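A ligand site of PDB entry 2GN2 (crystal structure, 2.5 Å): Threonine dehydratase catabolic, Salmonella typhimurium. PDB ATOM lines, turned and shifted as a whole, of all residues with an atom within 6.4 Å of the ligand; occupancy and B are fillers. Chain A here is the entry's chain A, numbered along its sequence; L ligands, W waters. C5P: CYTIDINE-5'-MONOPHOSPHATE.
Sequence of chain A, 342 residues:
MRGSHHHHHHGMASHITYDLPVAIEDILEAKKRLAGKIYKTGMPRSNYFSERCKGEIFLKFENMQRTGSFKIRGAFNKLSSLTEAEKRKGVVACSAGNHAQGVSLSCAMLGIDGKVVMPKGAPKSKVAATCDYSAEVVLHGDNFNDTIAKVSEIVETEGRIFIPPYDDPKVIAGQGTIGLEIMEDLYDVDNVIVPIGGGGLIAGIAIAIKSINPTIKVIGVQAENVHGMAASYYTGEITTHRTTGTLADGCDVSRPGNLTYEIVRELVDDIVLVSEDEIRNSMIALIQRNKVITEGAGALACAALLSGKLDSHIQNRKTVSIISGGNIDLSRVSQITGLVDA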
ATOM      1  N   ASN A  63     -22.566  29.630 -13.685  1.00  0.00           N
ATOM      2  CA  ASN A  63     -22.033  28.323 -14.096  1.00  0.00           C
ATOM      3  C   ASN A  63     -22.058  28.135 -15.615  1.00  0.00           C
ATOM      4  O   ASN A  63     -21.329  27.308 -16.152  1.00  0.00           O
ATOM      5  CB  ASN A  63     -22.751  27.161 -13.380  1.00  0.00           C
ATOM      6  CG  ASN A  63     -24.262  27.116 -13.636  1.00  0.00           C
ATOM      7  OD1 ASN A  63     -24.884  28.141 -13.917  1.00  0.00           O
ATOM      8  ND2 ASN A  63     -24.844  25.929 -13.492  1.00  0.00           N
ATOM      9  N   MET A  64     -22.886  28.906 -16.315  1.00  0.00           N
ATOM     10  CA  MET A  64     -22.942  28.845 -17.781  1.00  0.00           C
ATOM     11  C   MET A  64     -22.207  30.002 -18.429  1.00  0.00           C
ATOM     12  O   MET A  64     -22.287  30.216 -19.626  1.00  0.00           O
ATOM     13  CB  MET A  64     -24.393  28.751 -18.258  1.00  0.00           C
ATOM     14  CG  MET A  64     -25.129  27.605 -17.571  1.00  0.00           C
ATOM     15  SD  MET A  64     -26.765  27.285 -18.224  1.00  0.00           S
ATOM     16  CE  MET A  64     -27.332  25.973 -17.157  1.00  0.00           C
ATOM     17  N   GLN A  65     -21.470  30.756 -17.626  1.00  0.00           N
ATOM     18  CA  GLN A  65     -20.526  31.739 -18.157  1.00  0.00           C
ATOM     19  C   GLN A  65     -19.341  30.975 -18.743  1.00  0.00           C
ATOM     20  O   GLN A  65     -19.101  29.816 -18.364  1.00  0.00           O
ATOM     21  CB  GLN A  65     -20.097  32.690 -17.039  1.00  0.00           C
ATOM     22  CG  GLN A  65     -19.138  33.783 -17.448  1.00  0.00           C
ATOM     23  CD  GLN A  65     -19.674  34.630 -18.566  1.00  0.00           C
ATOM     24  OE1 GLN A  65     -19.380  34.387 -19.738  1.00  0.00           O
ATOM     25  NE2 GLN A  65     -20.492  35.612 -18.210  1.00  0.00           N
ATOM     26  N   ARG A  66     -18.611  31.590 -19.668  1.00  0.00           N
ATOM     27  CA  ARG A  66     -17.410  30.995 -20.252  1.00  0.00           C
ATOM     28  C   ARG A  66     -16.429  30.549 -19.151  1.00  0.00           C
ATOM     29  O   ARG A  66     -16.227  31.272 -18.157  1.00  0.00           O
ATOM     30  CB  ARG A  66     -16.731  31.976 -21.210  1.00  0.00           C
ATOM     31  CG  ARG A  66     -17.514  32.293 -22.499  1.00  0.00           C
ATOM     32  CD  ARG A  66     -17.821  31.033 -23.339  1.00  0.00           C
ATOM     33  NE  ARG A  66     -16.666  30.138 -23.481  1.00  0.00           N
ATOM     34  CZ  ARG A  66     -15.639  30.355 -24.310  1.00  0.00           C
ATOM     35  NH1 ARG A  66     -14.649  29.480 -24.360  1.00  0.00           N
ATOM     36  NH2 ARG A  66     -15.577  31.433 -25.074  1.00  0.00           N
ATOM     37  N   THR A  67     -15.838  29.360 -19.337  1.00  0.00           N
ATOM     38  CA  THR A  67     -14.935  28.672 -18.372  1.00  0.00           C
ATOM     39  C   THR A  67     -15.662  28.014 -17.200  1.00  0.00           C
ATOM     40  O   THR A  67     -15.044  27.270 -16.417  1.00  0.00           O
ATOM     41  CB  THR A  67     -13.801  29.563 -17.807  1.00  0.00           C
ATOM     42  OG1 THR A  67     -14.315  30.465 -16.829  1.00  0.00           O
ATOM     43  CG2 THR A  67     -13.120  30.346 -18.924  1.00  0.00           C
ATOM     44  N   GLY A  68     -16.966  28.262 -17.069  1.00  0.00           N
ATOM     45  CA  GLY A  68     -17.767  27.588 -16.059  1.00  0.00           C
ATOM     46  C   GLY A  68     -17.897  28.331 -14.747  1.00  0.00           C
ATOM     47  O   GLY A  68     -18.560  27.846 -13.830  1.00  0.00           O
ATOM     48  N   SER A  69     -17.269  29.497 -14.638  1.00  0.00           N
ATOM     49  CA  SER A  69     -17.530  30.390 -13.508  1.00  0.00           C
ATOM     50  C   SER A  69     -17.510  31.834 -13.957  1.00  0.00           C
ATOM     51  O   SER A  69     -17.251  32.155 -15.118  1.00  0.00           O
ATOM     52  CB  SER A  69     -16.536  30.155 -12.370  1.00  0.00           C
ATOM     53  OG  SER A  69     -15.307  30.813 -12.593  1.00  0.00           O
ATOM     54  N   ASN A  98     -10.728  28.056 -10.734  1.00  0.00           N
ATOM     55  CA  ASN A  98     -11.457  28.836 -11.723  1.00  0.00           C
ATOM     56  C   ASN A  98     -10.753  30.121 -12.173  1.00  0.00           C
ATOM     57  O   ASN A  98     -10.882  30.515 -13.330  1.00  0.00           O
ATOM     58  CB  ASN A  98     -12.873  29.111 -11.195  1.00  0.00           C
ATOM     59  CG  ASN A  98     -13.678  27.815 -10.987  1.00  0.00           C
ATOM     60  OD1 ASN A  98     -13.450  26.794 -11.650  1.00  0.00           O
ATOM     61  ND2 ASN A  98     -14.618  27.857 -10.053  1.00  0.00           N
ATOM     62  N   GLN A 101      -8.423  29.379 -15.021  1.00  0.00           N
ATOM     63  CA  GLN A 101      -9.162  29.254 -16.282  1.00  0.00           C
ATOM     64  C   GLN A 101      -9.531  30.607 -16.867  1.00  0.00           C
ATOM     65  O   GLN A 101      -9.390  30.816 -18.069  1.00  0.00           O
ATOM     66  CB  GLN A 101     -10.411  28.379 -16.092  1.00  0.00           C
ATOM     67  CG  GLN A 101     -10.085  27.019 -15.418  1.00  0.00           C
ATOM     68  CD  GLN A 101     -11.151  25.944 -15.571  1.00  0.00           C
ATOM     69  OE1 GLN A 101     -12.183  26.139 -16.208  1.00  0.00           O
ATOM     70  NE2 GLN A 101     -10.893  24.783 -14.977  1.00  0.00           N
ATOM     71  N   LEU A 105      -8.093  31.942 -20.442  1.00  0.00           N
ATOM     72  CA  LEU A 105      -8.980  32.303 -21.558  1.00  0.00           C
ATOM     73  C   LEU A 105      -8.885  33.783 -21.933  1.00  0.00           C
ATOM     74  O   LEU A 105      -8.845  34.118 -23.117  1.00  0.00           O
ATOM     75  CB  LEU A 105     -10.444  31.960 -21.272  1.00  0.00           C
ATOM     76  CG  LEU A 105     -11.427  32.362 -22.396  1.00  0.00           C
ATOM     77  CD1 LEU A 105     -11.066  31.688 -23.730  1.00  0.00           C
ATOM     78  CD2 LEU A 105     -12.848  32.041 -22.014  1.00  0.00           C
ATOM     79  N   SER A 125      -8.391  17.828 -13.819  1.00  0.00           N
ATOM     80  CA  SER A 125      -9.341  18.456 -14.734  1.00  0.00           C
ATOM     81  C   SER A 125      -9.076  19.951 -14.925  1.00  0.00           C
ATOM     82  O   SER A 125      -9.202  20.479 -16.038  1.00  0.00           O
ATOM     83  CB  SER A 125     -10.770  18.297 -14.185  1.00  0.00           C
ATOM     84  OG  SER A 125     -10.930  19.032 -12.978  1.00  0.00           O
ATOM     85  N   ALA A 128      -5.767  20.580 -16.867  1.00  0.00           N
ATOM     86  CA  ALA A 128      -6.026  20.330 -18.288  1.00  0.00           C
ATOM     87  C   ALA A 128      -6.827  21.466 -18.930  1.00  0.00           C
ATOM     88  O   ALA A 128      -6.506  21.919 -20.032  1.00  0.00           O
ATOM     89  CB  ALA A 128      -6.741  19.007 -18.486  1.00  0.00           C
ATOM     90  N   ALA A 129      -7.844  21.936 -18.238  1.00  0.00           N
ATOM     91  CA  ALA A 129      -8.688  22.983 -18.795  1.00  0.00           C
ATOM     92  C   ALA A 129      -7.893  24.277 -19.023  1.00  0.00           C
ATOM     93  O   ALA A 129      -8.021  24.901 -20.084  1.00  0.00           O
ATOM     94  CB  ALA A 129      -9.867  23.239 -17.893  1.00  0.00           C
ATOM     95  N   THR A 130      -7.044  24.664 -18.070  1.00  0.00           N
ATOM     96  CA  THR A 130      -6.315  25.934 -18.221  1.00  0.00           C
ATOM     97  C   THR A 130      -5.220  25.812 -19.282  1.00  0.00           C
ATOM     98  O   THR A 130      -4.849  26.818 -19.904  1.00  0.00           O
ATOM     99  CB  THR A 130      -5.724  26.534 -16.900  1.00  0.00           C
ATOM    100  OG1 THR A 130      -4.318  26.338 -16.868  1.00  0.00           O
ATOM    101  CG2 THR A 130      -6.344  25.966 -15.664  1.00  0.00           C
ATOM    102  N   ASP A 132      -5.880  24.018 -22.030  1.00  0.00           N
ATOM    103  CA  ASP A 132      -6.674  24.136 -23.238  1.00  0.00           C
ATOM    104  C   ASP A 132      -6.852  25.599 -23.578  1.00  0.00           C
ATOM    105  O   ASP A 132      -6.810  25.960 -24.742  1.00  0.00           O
ATOM    106  CB  ASP A 132      -8.041  23.446 -23.082  1.00  0.00           C
ATOM    107  CG  ASP A 132      -8.635  23.027 -24.438  1.00  0.00           C
ATOM    108  OD1 ASP A 132      -8.044  23.327 -25.488  1.00  0.00           O
ATOM    109  OD2 ASP A 132      -9.704  22.378 -24.435  1.00  0.00           O
ATOM    110  N   TYR A 133      -6.994  26.439 -22.562  1.00  0.00           N
ATOM    111  CA  TYR A 133      -7.259  27.870 -22.772  1.00  0.00           C
ATOM    112  C   TYR A 133      -6.038  28.711 -23.201  1.00  0.00           C
ATOM    113  O   TYR A 133      -6.169  29.914 -23.369  1.00  0.00           O
ATOM    114  CB  TYR A 133      -7.918  28.464 -21.537  1.00  0.00           C
ATOM    115  CG  TYR A 133      -9.343  27.989 -21.302  1.00  0.00           C
ATOM    116  CD1 TYR A 133      -9.728  27.487 -20.064  1.00  0.00           C
ATOM    117  CD2 TYR A 133     -10.298  28.058 -22.305  1.00  0.00           C
ATOM    118  CE1 TYR A 133     -11.021  27.057 -19.848  1.00  0.00           C
ATOM    119  CE2 TYR A 133     -11.591  27.611 -22.090  1.00  0.00           C
ATOM    120  CZ  TYR A 133     -11.942  27.116 -20.861  1.00  0.00           C
ATOM    121  OH  TYR A 133     -13.219  26.695 -20.629  1.00  0.00           O
ATOM    122  N   GLY A 326     -19.844  26.038 -11.970  1.00  0.00           N
ATOM    123  CA  GLY A 326     -20.210  24.656 -12.231  1.00  0.00           C
ATOM    124  C   GLY A 326     -19.019  23.741 -12.469  1.00  0.00           C
ATOM    125  O   GLY A 326     -19.174  22.668 -13.030  1.00  0.00           O
ATOM    126  N   ASN A 327     -17.829  24.144 -12.001  1.00  0.00           N
ATOM    127  CA  ASN A 327     -16.602  23.396 -12.261  1.00  0.00           C
ATOM    128  C   ASN A 327     -16.309  22.348 -11.176  1.00  0.00           C
ATOM    129  O   ASN A 327     -15.555  22.566 -10.226  1.00  0.00           O
ATOM    130  CB  ASN A 327     -15.426  24.347 -12.491  1.00  0.00           C
ATOM    131  CG  ASN A 327     -15.586  25.168 -13.772  1.00  0.00           C
ATOM    132  OD1 ASN A 327     -16.346  24.783 -14.659  1.00  0.00           O
ATOM    133  ND2 ASN A 327     -14.888  26.284 -13.874  1.00  0.00           N
HETATM  134  O3P C5P L   1     -17.156  27.784 -21.767  1.00  0.00           O
HETATM  135  P   C5P L   1     -16.275  26.711 -22.289  1.00  0.00           P
HETATM  136  O1P C5P L   1     -16.931  26.056 -23.482  1.00  0.00           O
HETATM  137  O2P C5P L   1     -14.896  27.273 -22.528  1.00  0.00           O
HETATM  138  O5' C5P L   1     -16.131  25.620 -21.116  1.00  0.00           O
HETATM  139  C5' C5P L   1     -17.317  25.000 -20.602  1.00  0.00           C
HETATM  140  C4' C5P L   1     -16.972  24.058 -19.442  1.00  0.00           C
HETATM  141  O4' C5P L   1     -16.057  23.058 -19.871  1.00  0.00           O
HETATM  142  C3' C5P L   1     -16.315  24.786 -18.276  1.00  0.00           C
HETATM  143  O3' C5P L   1     -16.822  24.312 -17.035  1.00  0.00           O
HETATM  144  C2' C5P L   1     -14.853  24.418 -18.378  1.00  0.00           C
HETATM  145  O2' C5P L   1     -14.190  24.397 -17.123  1.00  0.00           O
HETATM  146  C1' C5P L   1     -14.941  23.024 -18.977  1.00  0.00           C
HETATM  147  N1  C5P L   1     -13.718  22.597 -19.673  1.00  0.00           N
HETATM  148  C2  C5P L   1     -13.189  21.326 -19.389  1.00  0.00           C
HETATM  149  N3  C5P L   1     -12.083  20.893 -20.009  1.00  0.00           N
HETATM  150  C4  C5P L   1     -11.486  21.687 -20.928  1.00  0.00           C
HETATM  151  C5  C5P L   1     -11.990  22.951 -21.234  1.00  0.00           C
HETATM  152  C6  C5P L   1     -13.133  23.379 -20.583  1.00  0.00           C
HETATM  153  O2  C5P L   1     -13.735  20.585 -18.549  1.00  0.00           O
HETATM  154  N4  C5P L   1     -10.371  21.253 -21.538  1.00  0.00           N
HETATM  155  O   HOH W   1     -13.318  25.451 -24.301  1.00  0.00           O
HETATM  156  O   HOH W   2     -19.572  25.340 -23.432  1.00  0.00           O
HETATM  157  O   HOH W   3     -15.408  23.793 -24.139  1.00  0.00           O
HETATM  158  O   HOH W   4     -19.711  27.793 -21.297  1.00  0.00           O
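O of Thr 67 sits close to OE1 of Gln 101, 3.1 Å away.
The side-chain amide nitrogen (ND2) of Asn 327 sits at hydrogen-bond distance from the backbone carbonyl oxygen (O) of Thr 67 (2.7 Å).
OD1 of Asn 98 sits at hydrogen-bond distance from ND2 of Asn 327 (2.7 Å).
The backbone carbonyl oxygen (O) of Gly 68 lies within hydrogen-bond range of the backbone NH (N) of Gly 326 (2.9 Å).
Residues that only touch the ligand: Gly 68 and Ala 129.
Hydrophobic or aromatic side chains that line the ligand: Ala 129 and Tyr 133.
Eight residues have an atom within 4 Å of the ligand: Arg 66, Thr 67, Gly 68, Gln 101, Ala 129, Asp 132, Tyr 133 and Asn 327.
The nearest printed residue that does not touch the ligand is Ala 128 (4.2 Å).
N4 of the ligand sits at hydrogen-bond distance from OD2 of Asp 132 (3.2 Å).
The guanidinium group of Arg 66 is in salt-bridge range of an oxygen (O2P) of the ligand.
An oxygen (O3P) of the ligand sits at hydrogen-bond distance from the backbone NH (N) of Thr 67 (3.2 Å).
The backbone carbonyl oxygen (O) of Thr 67 lies within hydrogen-bond range of an oxygen (O2') of the ligand, at 3.1 Å.
OD1 of Asn 327 is in hydrogen-bond range of O3' of the ligand.
OH of Tyr 133 is in hydrogen-bond range of O2P of the ligand (2.6 Å).
An oxygen (O2') of the ligand is in hydrogen-bond range of the side-chain amide oxygen (OE1) of Gln 101, 2.8 Å away.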
